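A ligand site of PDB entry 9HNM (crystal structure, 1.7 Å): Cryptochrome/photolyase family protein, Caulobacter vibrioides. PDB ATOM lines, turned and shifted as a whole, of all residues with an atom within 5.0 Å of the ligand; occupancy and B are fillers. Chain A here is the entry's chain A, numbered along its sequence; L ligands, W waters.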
ATOM      1  N   PHE A 248       8.661 -16.948  10.266  1.00  0.00           N
ATOM      2  CA  PHE A 248       8.349 -17.420  11.601  1.00  0.00           C
ATOM      3  C   PHE A 248       8.716 -16.420  12.694  1.00  0.00           C
ATOM      4  O   PHE A 248       7.950 -16.207  13.649  1.00  0.00           O
ATOM      5  CB  PHE A 248       9.066 -18.750  11.833  1.00  0.00           C
ATOM      6  CG  PHE A 248       8.784 -19.344  13.190  1.00  0.00           C
ATOM      7  CD1 PHE A 248       7.584 -20.035  13.411  1.00  0.00           C
ATOM      8  CD2 PHE A 248       9.681 -19.199  14.232  1.00  0.00           C
ATOM      9  CE1 PHE A 248       7.284 -20.613  14.672  1.00  0.00           C
ATOM     10  CE2 PHE A 248       9.415 -19.770  15.506  1.00  0.00           C
ATOM     11  CZ  PHE A 248       8.182 -20.477  15.710  1.00  0.00           C
ATOM     12  N   HIS A 264       2.609 -20.254  12.545  1.00  0.00           N
ATOM     13  CA  HIS A 264       3.136 -21.335  13.377  1.00  0.00           C
ATOM     14  C   HIS A 264       3.176 -22.682  12.646  1.00  0.00           C
ATOM     15  O   HIS A 264       2.546 -22.872  11.590  1.00  0.00           O
ATOM     16  CB  HIS A 264       2.265 -21.437  14.661  1.00  0.00           C
ATOM     17  CG  HIS A 264       2.405 -20.200  15.502  1.00  0.00           C
ATOM     18  ND1 HIS A 264       3.441 -20.024  16.409  1.00  0.00           N
ATOM     19  CD2 HIS A 264       1.710 -19.032  15.513  1.00  0.00           C
ATOM     20  CE1 HIS A 264       3.362 -18.809  16.956  1.00  0.00           C
ATOM     21  NE2 HIS A 264       2.324 -18.178  16.415  1.00  0.00           N
ATOM     22  N   SER A 265       3.927 -23.646  13.197  1.00  0.00           N
ATOM     23  CA  SER A 265       4.154 -24.884  12.406  1.00  0.00           C
ATOM     24  C   SER A 265       2.984 -25.868  12.500  1.00  0.00           C
ATOM     25  O   SER A 265       2.800 -26.687  11.595  1.00  0.00           O
ATOM     26  CB  SER A 265       5.478 -25.561  12.835  1.00  0.00           C
ATOM     27  OG  SER A 265       5.372 -26.051  14.201  1.00  0.00           O
ATOM     28  N   LEU A 266       2.202 -25.802  13.577  1.00  0.00           N
ATOM     29  CA  LEU A 266       1.068 -26.699  13.791  1.00  0.00           C
ATOM     30  C   LEU A 266       1.529 -28.135  13.915  1.00  0.00           C
ATOM     31  O   LEU A 266       0.757 -29.051  13.582  1.00  0.00           O
ATOM     32  CB  LEU A 266       0.045 -26.618  12.646  1.00  0.00           C
ATOM     33  CG  LEU A 266      -0.308 -25.143  12.302  1.00  0.00           C
ATOM     34  CD1 LEU A 266      -1.527 -25.117  11.326  1.00  0.00           C
ATOM     35  CD2 LEU A 266      -0.626 -24.301  13.554  1.00  0.00           C
ATOM     36  N   ILE A 267       2.766 -28.355  14.390  1.00  0.00           N
ATOM     37  CA  ILE A 267       3.241 -29.750  14.440  1.00  0.00           C
ATOM     38  C   ILE A 267       3.126 -30.401  15.808  1.00  0.00           C
ATOM     39  O   ILE A 267       3.337 -31.623  15.910  1.00  0.00           O
ATOM     40  CB  ILE A 267       4.705 -29.921  13.962  1.00  0.00           C
ATOM     41  CG1 ILE A 267       5.632 -29.226  14.965  1.00  0.00           C
ATOM     42  CG2 ILE A 267       4.842 -29.502  12.501  1.00  0.00           C
ATOM     43  CD1 ILE A 267       7.105 -29.393  14.586  1.00  0.00           C
ATOM     44  N   SER A 268       2.769 -29.660  16.860  1.00  0.00           N
ATOM     45  CA  SER A 268       2.860 -30.274  18.177  1.00  0.00           C
ATOM     46  C   SER A 268       1.954 -31.494  18.313  1.00  0.00           C
ATOM     47  O   SER A 268       2.370 -32.447  19.013  1.00  0.00           O
ATOM     48  CB  SER A 268       2.590 -29.212  19.243  1.00  0.00           C
ATOM     49  OG  SER A 268       1.296 -28.622  19.064  1.00  0.00           O
ATOM     50  N   LEU A 271       4.035 -34.303  16.647  1.00  0.00           N
ATOM     51  CA  LEU A 271       5.306 -34.538  17.324  1.00  0.00           C
ATOM     52  C   LEU A 271       5.083 -35.242  18.663  1.00  0.00           C
ATOM     53  O   LEU A 271       5.824 -36.161  19.045  1.00  0.00           O
ATOM     54  CB  LEU A 271       6.001 -33.194  17.528  1.00  0.00           C
ATOM     55  CG  LEU A 271       7.352 -33.213  18.242  1.00  0.00           C
ATOM     56  CD1 LEU A 271       8.364 -34.134  17.587  1.00  0.00           C
ATOM     57  CD2 LEU A 271       7.917 -31.760  18.326  1.00  0.00           C
ATOM     58  N   ASN A 272       4.062 -34.813  19.404  1.00  0.00           N
ATOM     59  CA  ASN A 272       3.892 -35.377  20.747  1.00  0.00           C
ATOM     60  C   ASN A 272       3.391 -36.812  20.769  1.00  0.00           C
ATOM     61  O   ASN A 272       3.385 -37.414  21.858  1.00  0.00           O
ATOM     62  CB  ASN A 272       2.931 -34.454  21.515  1.00  0.00           C
ATOM     63  CG  ASN A 272       3.648 -33.192  21.980  1.00  0.00           C
ATOM     64  OD1 ASN A 272       4.867 -33.080  21.839  1.00  0.00           O
ATOM     65  ND2 ASN A 272       2.872 -32.250  22.559  1.00  0.00           N
ATOM     66  N   PHE A 302      12.872 -20.951  15.819  1.00  0.00           N
ATOM     67  CA  PHE A 302      12.128 -22.206  15.736  1.00  0.00           C
ATOM     68  C   PHE A 302      12.844 -23.328  16.531  1.00  0.00           C
ATOM     69  O   PHE A 302      12.212 -24.014  17.338  1.00  0.00           O
ATOM     70  CB  PHE A 302      11.988 -22.584  14.259  1.00  0.00           C
ATOM     71  CG  PHE A 302      11.259 -23.858  14.045  1.00  0.00           C
ATOM     72  CD1 PHE A 302       9.891 -23.944  14.279  1.00  0.00           C
ATOM     73  CD2 PHE A 302      11.927 -24.921  13.544  1.00  0.00           C
ATOM     74  CE1 PHE A 302       9.208 -25.162  14.056  1.00  0.00           C
ATOM     75  CE2 PHE A 302      11.282 -26.153  13.290  1.00  0.00           C
ATOM     76  CZ  PHE A 302       9.903 -26.287  13.546  1.00  0.00           C
ATOM     77  N   GLN A 305      12.595 -23.399  20.321  1.00  0.00           N
ATOM     78  CA  GLN A 305      11.346 -23.866  20.921  1.00  0.00           C
ATOM     79  C   GLN A 305      11.375 -25.377  21.122  1.00  0.00           C
ATOM     80  O   GLN A 305      10.738 -25.876  22.046  1.00  0.00           O
ATOM     81  CB  GLN A 305      10.128 -23.535  20.015  1.00  0.00           C
ATOM     82  CG  GLN A 305      10.039 -22.058  19.634  1.00  0.00           C
ATOM     83  CD  GLN A 305      10.302 -21.088  20.718  1.00  0.00           C
ATOM     84  OE1 GLN A 305       9.707 -21.238  21.807  1.00  0.00           O
ATOM     85  NE2 GLN A 305      11.236 -20.093  20.515  1.00  0.00           N
ATOM     86  N   ILE A 306      12.133 -26.097  20.278  1.00  0.00           N
ATOM     87  CA  ILE A 306      12.111 -27.560  20.296  1.00  0.00           C
ATOM     88  C   ILE A 306      13.235 -28.132  21.166  1.00  0.00           C
ATOM     89  O   ILE A 306      12.994 -29.029  22.014  1.00  0.00           O
ATOM     90  CB  ILE A 306      12.144 -28.092  18.840  1.00  0.00           C
ATOM     91  CG1 ILE A 306      10.851 -27.636  18.130  1.00  0.00           C
ATOM     92  CG2 ILE A 306      12.279 -29.661  18.874  1.00  0.00           C
ATOM     93  CD1 ILE A 306      10.917 -27.940  16.662  1.00  0.00           C
ATOM     94  N   TRP A 309      12.796 -25.024  24.808  1.00  0.00           N
ATOM     95  CA  TRP A 309      11.622 -25.092  25.697  1.00  0.00           C
ATOM     96  C   TRP A 309      11.092 -26.516  25.862  1.00  0.00           C
ATOM     97  O   TRP A 309      10.801 -26.944  26.995  1.00  0.00           O
ATOM     98  CB  TRP A 309      10.487 -24.178  25.228  1.00  0.00           C
ATOM     99  CG  TRP A 309      10.789 -22.764  25.669  1.00  0.00           C
ATOM    100  CD1 TRP A 309      11.086 -21.695  24.851  1.00  0.00           C
ATOM    101  CD2 TRP A 309      10.826 -22.260  27.021  1.00  0.00           C
ATOM    102  NE1 TRP A 309      11.316 -20.555  25.616  1.00  0.00           N
ATOM    103  CE2 TRP A 309      11.148 -20.869  26.941  1.00  0.00           C
ATOM    104  CE3 TRP A 309      10.620 -22.860  28.279  1.00  0.00           C
ATOM    105  CZ2 TRP A 309      11.265 -20.061  28.065  1.00  0.00           C
ATOM    106  CZ3 TRP A 309      10.737 -22.051  29.419  1.00  0.00           C
ATOM    107  CH2 TRP A 309      11.039 -20.662  29.298  1.00  0.00           C
ATOM    108  N   ARG A 310      10.933 -27.253  24.768  1.00  0.00           N
ATOM    109  CA  ARG A 310      10.246 -28.548  24.897  1.00  0.00           C
ATOM    110  C   ARG A 310      11.033 -29.519  25.743  1.00  0.00           C
ATOM    111  O   ARG A 310      10.464 -30.222  26.613  1.00  0.00           O
ATOM    112  CB  ARG A 310      10.013 -29.137  23.474  1.00  0.00           C
ATOM    113  CG  ARG A 310       9.160 -30.409  23.486  1.00  0.00           C
ATOM    114  CD  ARG A 310       8.886 -30.823  22.028  1.00  0.00           C
ATOM    115  NE  ARG A 310       8.006 -31.991  21.991  1.00  0.00           N
ATOM    116  CZ  ARG A 310       8.437 -33.246  21.860  1.00  0.00           C
ATOM    117  NH1 ARG A 310       9.708 -33.537  21.734  1.00  0.00           N
ATOM    118  NH2 ARG A 310       7.552 -34.256  21.805  1.00  0.00           N
ATOM    119  N   VAL A 313      10.952 -28.169  29.662  1.00  0.00           N
ATOM    120  CA  VAL A 313       9.782 -28.440  30.506  1.00  0.00           C
ATOM    121  C   VAL A 313       9.668 -29.918  30.829  1.00  0.00           C
ATOM    122  O   VAL A 313       9.266 -30.278  31.942  1.00  0.00           O
ATOM    123  CB  VAL A 313       8.517 -27.849  29.869  1.00  0.00           C
ATOM    124  CG1 VAL A 313       8.658 -26.335  29.654  1.00  0.00           C
ATOM    125  CG2 VAL A 313       7.994 -28.625  28.567  1.00  0.00           C
ATOM    126  N   TYR A 362      -6.691 -26.117  19.128  1.00  0.00           N
ATOM    127  CA  TYR A 362      -5.385 -25.491  19.025  1.00  0.00           C
ATOM    128  C   TYR A 362      -5.486 -24.013  19.313  1.00  0.00           C
ATOM    129  O   TYR A 362      -6.454 -23.365  18.902  1.00  0.00           O
ATOM    130  CB  TYR A 362      -4.850 -25.635  17.583  1.00  0.00           C
ATOM    131  CG  TYR A 362      -3.546 -24.903  17.345  1.00  0.00           C
ATOM    132  CD1 TYR A 362      -3.537 -23.573  16.917  1.00  0.00           C
ATOM    133  CD2 TYR A 362      -2.323 -25.539  17.594  1.00  0.00           C
ATOM    134  CE1 TYR A 362      -2.334 -22.909  16.681  1.00  0.00           C
ATOM    135  CE2 TYR A 362      -1.102 -24.864  17.405  1.00  0.00           C
ATOM    136  CZ  TYR A 362      -1.132 -23.557  16.948  1.00  0.00           C
ATOM    137  OH  TYR A 362       0.062 -22.946  16.684  1.00  0.00           O
ATOM    138  N   ALA A 363      -4.473 -23.484  19.985  1.00  0.00           N
ATOM    139  CA  ALA A 363      -4.244 -22.048  19.994  1.00  0.00           C
ATOM    140  C   ALA A 363      -2.746 -21.924  20.094  1.00  0.00           C
ATOM    141  O   ALA A 363      -2.096 -22.804  20.683  1.00  0.00           O
ATOM    142  CB  ALA A 363      -4.940 -21.341  21.210  1.00  0.00           C
ATOM    143  N   HIS A 364      -2.176 -20.818  19.596  1.00  0.00           N
ATOM    144  CA  HIS A 364      -0.734 -20.765  19.650  1.00  0.00           C
ATOM    145  C   HIS A 364      -0.231 -20.220  20.995  1.00  0.00           C
ATOM    146  O   HIS A 364      -1.009 -19.912  21.898  1.00  0.00           O
ATOM    147  CB  HIS A 364      -0.170 -19.963  18.447  1.00  0.00           C
ATOM    148  CG  HIS A 364      -0.693 -18.560  18.329  1.00  0.00           C
ATOM    149  ND1 HIS A 364      -0.228 -17.519  19.091  1.00  0.00           N
ATOM    150  CD2 HIS A 364      -1.581 -18.007  17.457  1.00  0.00           C
ATOM    151  CE1 HIS A 364      -0.831 -16.390  18.726  1.00  0.00           C
ATOM    152  NE2 HIS A 364      -1.671 -16.667  17.750  1.00  0.00           N
ATOM    153  N   HIS A 365       1.097 -20.237  21.155  1.00  0.00           N
ATOM    154  CA  HIS A 365       1.720 -20.124  22.476  1.00  0.00           C
ATOM    155  C   HIS A 365       1.322 -18.832  23.199  1.00  0.00           C
ATOM    156  O   HIS A 365       0.901 -18.872  24.349  1.00  0.00           O
ATOM    157  CB  HIS A 365       3.254 -20.234  22.361  1.00  0.00           C
ATOM    158  CG  HIS A 365       3.952 -20.078  23.681  1.00  0.00           C
ATOM    159  ND1 HIS A 365       3.953 -21.064  24.658  1.00  0.00           N
ATOM    160  CD2 HIS A 365       4.664 -19.039  24.178  1.00  0.00           C
ATOM    161  CE1 HIS A 365       4.674 -20.654  25.682  1.00  0.00           C
ATOM    162  NE2 HIS A 365       5.124 -19.421  25.413  1.00  0.00           N
ATOM    163  N   ARG A 368      -2.248 -18.928  24.501  1.00  0.00           N
ATOM    164  CA  ARG A 368      -2.384 -19.756  25.708  1.00  0.00           C
ATOM    165  C   ARG A 368      -1.765 -19.067  26.915  1.00  0.00           C
ATOM    166  O   ARG A 368      -2.252 -19.250  28.043  1.00  0.00           O
ATOM    167  CB  ARG A 368      -1.667 -21.107  25.534  1.00  0.00           C
ATOM    168  CG  ARG A 368      -2.291 -21.983  24.418  1.00  0.00           C
ATOM    169  CD  ARG A 368      -1.734 -23.466  24.542  1.00  0.00           C
ATOM    170  NE  ARG A 368      -1.746 -24.022  23.185  1.00  0.00           N
ATOM    171  CZ  ARG A 368      -1.498 -25.296  22.906  1.00  0.00           C
ATOM    172  NH1 ARG A 368      -1.425 -26.207  23.884  1.00  0.00           N
ATOM    173  NH2 ARG A 368      -1.331 -25.641  21.617  1.00  0.00           N
ATOM    174  N   LEU A 369      -0.684 -18.311  26.696  1.00  0.00           N
ATOM    175  CA  LEU A 369       0.031 -17.700  27.813  1.00  0.00           C
ATOM    176  C   LEU A 369      -0.622 -16.413  28.243  1.00  0.00           C
ATOM    177  O   LEU A 369      -0.921 -16.233  29.433  1.00  0.00           O
ATOM    178  CB  LEU A 369       1.496 -17.398  27.431  1.00  0.00           C
ATOM    179  CG  LEU A 369       2.429 -16.784  28.438  1.00  0.00           C
ATOM    180  CD1 LEU A 369       2.560 -17.678  29.668  1.00  0.00           C
ATOM    181  CD2 LEU A 369       3.850 -16.477  27.785  1.00  0.00           C
ATOM    182  N   TYR A 390      -6.532 -26.854  30.373  1.00  0.00           N
ATOM    183  CA  TYR A 390      -5.478 -26.983  29.360  1.00  0.00           C
ATOM    184  C   TYR A 390      -5.282 -28.432  28.952  1.00  0.00           C
ATOM    185  O   TYR A 390      -4.839 -28.670  27.812  1.00  0.00           O
ATOM    186  CB  TYR A 390      -4.148 -26.433  29.884  1.00  0.00           C
ATOM    187  CG  TYR A 390      -4.099 -24.927  29.688  1.00  0.00           C
ATOM    188  CD1 TYR A 390      -3.643 -24.388  28.487  1.00  0.00           C
ATOM    189  CD2 TYR A 390      -4.599 -24.044  30.680  1.00  0.00           C
ATOM    190  CE1 TYR A 390      -3.698 -22.979  28.238  1.00  0.00           C
ATOM    191  CE2 TYR A 390      -4.605 -22.655  30.477  1.00  0.00           C
ATOM    192  CZ  TYR A 390      -4.141 -22.120  29.265  1.00  0.00           C
ATOM    193  OH  TYR A 390      -4.205 -20.732  29.094  1.00  0.00           O
ATOM    194  N   ASP A 396      -2.602 -31.202  21.598  1.00  0.00           N
ATOM    195  CA  ASP A 396      -1.201 -31.502  21.894  1.00  0.00           C
ATOM    196  C   ASP A 396      -0.969 -31.687  23.396  1.00  0.00           C
ATOM    197  O   ASP A 396       0.182 -31.776  23.822  1.00  0.00           O
ATOM    198  CB  ASP A 396      -0.252 -30.389  21.330  1.00  0.00           C
ATOM    199  CG  ASP A 396      -0.555 -29.026  21.875  1.00  0.00           C
ATOM    200  OD1 ASP A 396      -1.368 -28.918  22.806  1.00  0.00           O
ATOM    201  OD2 ASP A 396       0.044 -28.020  21.379  1.00  0.00           O
ATOM    202  N   ALA A 397      -2.021 -31.791  24.186  1.00  0.00           N
ATOM    203  CA  ALA A 397      -1.874 -31.757  25.646  1.00  0.00           C
ATOM    204  C   ALA A 397      -1.624 -33.144  26.230  1.00  0.00           C
ATOM    205  O   ALA A 397      -2.432 -34.096  26.103  1.00  0.00           O
ATOM    206  CB  ALA A 397      -3.117 -31.069  26.310  1.00  0.00           C
ATOM    207  N   TYR A 398      -0.451 -33.295  26.880  1.00  0.00           N
ATOM    208  CA  TYR A 398      -0.061 -34.438  27.694  1.00  0.00           C
ATOM    209  C   TYR A 398       0.558 -33.870  28.955  1.00  0.00           C
ATOM    210  O   TYR A 398       1.083 -32.741  28.912  1.00  0.00           O
ATOM    211  CB  TYR A 398       0.984 -35.339  26.921  1.00  0.00           C
ATOM    212  CG  TYR A 398       0.366 -35.837  25.657  1.00  0.00           C
ATOM    213  CD1 TYR A 398      -0.416 -37.002  25.655  1.00  0.00           C
ATOM    214  CD2 TYR A 398       0.471 -35.085  24.481  1.00  0.00           C
ATOM    215  CE1 TYR A 398      -1.038 -37.425  24.504  1.00  0.00           C
ATOM    216  CE2 TYR A 398      -0.252 -35.467  23.320  1.00  0.00           C
ATOM    217  CZ  TYR A 398      -0.979 -36.655  23.370  1.00  0.00           C
ATOM    218  OH  TYR A 398      -1.705 -37.132  22.277  1.00  0.00           O
ATOM    219  N   VAL A 401       4.072 -31.990  29.322  1.00  0.00           N
ATOM    220  CA  VAL A 401       4.304 -30.718  28.663  1.00  0.00           C
ATOM    221  C   VAL A 401       3.279 -29.669  29.082  1.00  0.00           C
ATOM    222  O   VAL A 401       3.604 -28.486  29.259  1.00  0.00           O
ATOM    223  CB  VAL A 401       4.372 -30.919  27.130  1.00  0.00           C
ATOM    224  CG1 VAL A 401       3.122 -31.560  26.557  1.00  0.00           C
ATOM    225  CG2 VAL A 401       4.678 -29.527  26.351  1.00  0.00           C
ATOM    226  N   GLU A 402       2.022 -30.092  29.327  1.00  0.00           N
ATOM    227  CA  GLU A 402       1.009 -29.140  29.798  1.00  0.00           C
ATOM    228  C   GLU A 402       1.358 -28.541  31.163  1.00  0.00           C
ATOM    229  O   GLU A 402       1.280 -27.309  31.381  1.00  0.00           O
ATOM    230  CB  GLU A 402      -0.346 -29.853  29.885  1.00  0.00           C
ATOM    231  CG  GLU A 402      -1.542 -28.997  30.479  1.00  0.00           C
ATOM    232  CD  GLU A 402      -1.551 -29.000  31.998  1.00  0.00           C
ATOM    233  OE1 GLU A 402      -1.295 -30.061  32.655  1.00  0.00           O
ATOM    234  OE2 GLU A 402      -1.854 -27.913  32.547  1.00  0.00           O
ATOM    235  N   ASN A 405       4.132 -25.830  31.687  1.00  0.00           N
ATOM    236  CA  ASN A 405       3.768 -24.620  30.966  1.00  0.00           C
ATOM    237  C   ASN A 405       2.609 -23.910  31.626  1.00  0.00           C
ATOM    238  O   ASN A 405       2.491 -22.689  31.500  1.00  0.00           O
ATOM    239  CB  ASN A 405       3.359 -24.943  29.525  1.00  0.00           C
ATOM    240  CG  ASN A 405       4.589 -25.032  28.599  1.00  0.00           C
ATOM    241  OD1 ASN A 405       5.303 -24.056  28.409  1.00  0.00           O
ATOM    242  ND2 ASN A 405       4.810 -26.213  27.975  1.00  0.00           N
ATOM    243  N   THR A 406       1.754 -24.665  32.305  1.00  0.00           N
ATOM    244  CA  THR A 406       0.512 -24.085  32.830  1.00  0.00           C
ATOM    245  C   THR A 406       0.628 -23.773  34.320  1.00  0.00           C
ATOM    246  O   THR A 406       0.510 -22.590  34.728  1.00  0.00           O
ATOM    247  CB  THR A 406      -0.657 -25.061  32.574  1.00  0.00           C
ATOM    248  OG1 THR A 406      -0.679 -25.357  31.157  1.00  0.00           O
ATOM    249  CG2 THR A 406      -2.000 -24.402  32.996  1.00  0.00           C
ATOM    250  N   MET A 409       4.707 -21.763  33.819  1.00  0.00           N
ATOM    251  CA  MET A 409       4.989 -20.501  33.147  1.00  0.00           C
ATOM    252  C   MET A 409       3.773 -19.562  33.142  1.00  0.00           C
ATOM    253  O   MET A 409       3.914 -18.358  33.435  1.00  0.00           O
ATOM    254  CB  MET A 409       5.570 -20.804  31.754  1.00  0.00           C
ATOM    255  CG  MET A 409       6.022 -19.600  30.906  1.00  0.00           C
ATOM    256  SD  MET A 409       6.051 -19.961  29.133  1.00  0.00           S
ATOM    257  CE  MET A 409       7.273 -21.261  29.006  1.00  0.00           C
ATOM    258  N   ALA A 410       2.568 -20.090  32.936  1.00  0.00           N
ATOM    259  CA  ALA A 410       1.436 -19.187  32.719  1.00  0.00           C
ATOM    260  C   ALA A 410       0.824 -18.696  34.012  1.00  0.00           C
ATOM    261  O   ALA A 410       0.260 -17.569  34.017  1.00  0.00           O
ATOM    262  CB  ALA A 410       0.314 -19.866  31.901  1.00  0.00           C
HETATM  263  P1  LIG L   1       5.355 -23.459  17.001  1.00  0.00           P
HETATM  264  O1  LIG L   1       5.013 -22.078  17.443  1.00  0.00           O
HETATM  265  O2  LIG L   1       5.452 -23.687  15.502  1.00  0.00           O
HETATM  266  O3  LIG L   1       6.624 -23.970  17.850  1.00  0.00           O
HETATM  267  C1  LIG L   1       7.396 -25.093  17.350  1.00  0.00           C
HETATM  268  C2  LIG L   1       7.445 -26.236  18.330  1.00  0.00           C
HETATM  269  O4  LIG L   1       8.120 -25.803  19.535  1.00  0.00           O
HETATM  270  C3  LIG L   1       6.096 -26.742  18.836  1.00  0.00           C
HETATM  271  O5  LIG L   1       5.544 -27.624  17.871  1.00  0.00           O
HETATM  272  C4  LIG L   1       6.516 -27.464  20.120  1.00  0.00           C
HETATM  273  O6  LIG L   1       7.120 -28.718  19.789  1.00  0.00           O
HETATM  274  C5  LIG L   1       7.630 -26.588  20.635  1.00  0.00           C
HETATM  275  N1  LIG L   1       7.245 -25.661  21.675  1.00  0.00           N
HETATM  276  C6  LIG L   1       7.068 -24.308  21.548  1.00  0.00           C
HETATM  277  N2  LIG L   1       6.830 -23.696  22.691  1.00  0.00           N
HETATM  278  C7  LIG L   1       6.893 -24.725  23.630  1.00  0.00           C
HETATM  279  C8  LIG L   1       6.755 -24.738  25.038  1.00  0.00           C
HETATM  280  N3  LIG L   1       6.557 -23.646  25.767  1.00  0.00           N
HETATM  281  N4  LIG L   1       6.845 -25.925  25.665  1.00  0.00           N
HETATM  282  C9  LIG L   1       7.066 -27.028  24.939  1.00  0.00           C
HETATM  283  N5  LIG L   1       7.225 -27.144  23.605  1.00  0.00           N
HETATM  284  C10 LIG L   1       7.131 -25.944  23.017  1.00  0.00           C
HETATM  285  N6  LIG L   1       2.737 -27.439  24.214  1.00  0.00           N
HETATM  286  C11 LIG L   1       2.373 -28.740  23.996  1.00  0.00           C
HETATM  287  O7  LIG L   1       2.958 -29.425  23.137  1.00  0.00           O
HETATM  288  N7  LIG L   1       1.402 -29.327  24.765  1.00  0.00           N
HETATM  289  C12 LIG L   1       0.686 -28.686  25.761  1.00  0.00           C
HETATM  290  O8  LIG L   1      -0.114 -29.310  26.423  1.00  0.00           O
HETATM  291  C13 LIG L   1       1.066 -27.313  25.978  1.00  0.00           C
HETATM  292  N8  LIG L   1       0.429 -26.637  26.905  1.00  0.00           N
HETATM  293  C14 LIG L   1       0.717 -25.306  27.034  1.00  0.00           C
HETATM  294  C15 LIG L   1      -0.010 -24.590  27.997  1.00  0.00           C
HETATM  295  C16 LIG L   1       0.265 -23.251  28.235  1.00  0.00           C
HETATM  296  C17 LIG L   1      -0.499 -22.522  29.335  1.00  0.00           C
HETATM  297  C18 LIG L   1       1.281 -22.620  27.498  1.00  0.00           C
HETATM  298  C19 LIG L   1       1.604 -21.158  27.707  1.00  0.00           C
HETATM  299  C20 LIG L   1       2.000 -23.317  26.521  1.00  0.00           C
HETATM  300  C21 LIG L   1       1.698 -24.660  26.264  1.00  0.00           C
HETATM  301  N9  LIG L   1       2.366 -25.421  25.267  1.00  0.00           N
HETATM  302  C22 LIG L   1       2.065 -26.755  25.120  1.00  0.00           C
HETATM  303  C23 LIG L   1       3.526 -24.866  24.466  1.00  0.00           C
HETATM  304  C24 LIG L   1       3.133 -24.185  23.135  1.00  0.00           C
HETATM  305  O9  LIG L   1       2.043 -23.306  23.413  1.00  0.00           O
HETATM  306  C25 LIG L   1       2.748 -25.256  22.109  1.00  0.00           C
HETATM  307  O10 LIG L   1       3.820 -26.184  21.982  1.00  0.00           O
HETATM  308  C26 LIG L   1       2.531 -24.618  20.724  1.00  0.00           C
HETATM  309  O11 LIG L   1       1.484 -23.635  20.817  1.00  0.00           O
HETATM  310  C27 LIG L   1       2.222 -25.636  19.654  1.00  0.00           C
HETATM  311  O12 LIG L   1       2.001 -24.945  18.402  1.00  0.00           O
HETATM  312  P2  LIG L   1       2.918 -25.165  17.130  1.00  0.00           P
HETATM  313  O13 LIG L   1       3.226 -26.628  16.917  1.00  0.00           O
HETATM  314  O14 LIG L   1       2.221 -24.392  16.057  1.00  0.00           O
HETATM  315  O15 LIG L   1       4.276 -24.475  17.593  1.00  0.00           O
HETATM  316  O   HOH W   1       2.557 -21.793  19.016  1.00  0.00           O
HETATM  317  O   HOH W   2       6.957 -20.897  22.483  1.00  0.00           O
HETATM  318  O   HOH W   3       6.162 -20.044  19.199  1.00  0.00           O
HETATM  319  O   HOH W   4      -2.523 -27.276  26.717  1.00  0.00           O
HETATM  320  O   HOH W   5       5.715 -29.711  22.677  1.00  0.00           O
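Merely in contact with the ligand: Phe 248, Leu 271, Phe 302, Gln 305, Ile 306, Trp 309, Arg 310, Ala 363, His 364, Arg 368, Leu 369, Tyr 390, Ala 397, Val 401, Glu 402, Thr 406 and Ala 410. Hydrophobic or aromatic side chains within 4 Å of the ligand: Phe 248, His 264, Leu 266, Ile 267, Leu 271, Phe 302, Ile 306, Trp 309, Tyr 362, His 365, Leu 369, Tyr 390, Ala 397, Val 401 and Ala 410. Of the 30 residues printed, 27 come within 4 Å of the ligand. The nearest printed residue that does not touch the ligand is Tyr 398 (4.03 Å).
The guanidinium group (NH2) of Arg 368 is in salt-bridge range of the side-chain carboxylate (OD2) of Asp 396. O of Arg 368 is in hydrogen-bond range of OH of Tyr 390. The backbone carbonyl oxygen (O) of Val 401 is in hydrogen-bond range of the side-chain amide nitrogen (ND2) of Asn 405 (2.9 Å). OG1 of Thr 406 lies within hydrogen-bond range of O of Glu 402. The backbone NH (N) of Ile 267 sits close to the side-chain hydroxyl (OG) of Ser 265, 3.5 Å away. The side-chain hydroxyl of Ser 268 is in hydrogen-bond range of the side-chain carboxylate of Asp 396, 2.7 Å away. The backbone carbonyl oxygen of Gln 305 sits at hydrogen-bond distance from the backbone NH of Arg 310 (3.1 Å). O of Asn 405 lies within hydrogen-bond range of N of Ala 410 (3.0 Å).
Water W1 lies within hydrogen-bond range of O11 of the ligand (2.8 Å), N of His 365 (3.0 Å) and ND1 of His 264 (3.3 Å). Water W5 bridges an oxygen (O7) of the ligand (2.8 Å) and the guanidinium group (NE) of Arg 310 (3.3 Å). Water W2 bridges a nitrogen (N2) of the ligand (2.8 Å) and the side-chain amide oxygen of Gln 305 (2.9 Å). Water W4 lies within hydrogen-bond range of O of Tyr 390, N8 of the ligand and NH1 of Arg 368.
A ring nitrogen (ND1) of His 365 lies within hydrogen-bond range of an oxygen (O9) of the ligand (3.2 Å). A nitrogen (N3) of the ligand is in hydrogen-bond range of the side-chain amide oxygen (OD1) of Asn 405. N of Ser 265 sits at hydrogen-bond distance from O2 of the ligand (2.8 Å). An oxygen (O7) of the ligand is in hydrogen-bond range of the side-chain amide nitrogen (ND2) of Asn 272, at 2.9 Å. A nitrogen (N7) of the ligand sits at hydrogen-bond distance from the backbone carbonyl oxygen (O) of Asp 396, at 2.9 Å. A nitrogen (N7) of the ligand sits at hydrogen-bond distance from the side-chain carboxylate (OD1) of Asp 396, at 3.4 Å. N of Ser 268 sits at hydrogen-bond distance from O13 of the ligand (3.1 Å). N of Ile 267 is in hydrogen-bond range of O13 of the ligand (3.1 Å). An oxygen (O11) of the ligand sits at hydrogen-bond distance from the backbone NH (N) of His 365 (3.4 Å). O2 of the ligand is in hydrogen-bond range of OG of Ser 265 (2.7 Å). An oxygen (O14) of the ligand sits at hydrogen-bond distance from the side-chain hydroxyl of Tyr 362, at 2.7 Å. An oxygen (O14) of the ligand sits at hydrogen-bond distance from the backbone NH of Leu 266 (2.9 Å). ND1 of His 264 lies within hydrogen-bond range of O1 of the ligand.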
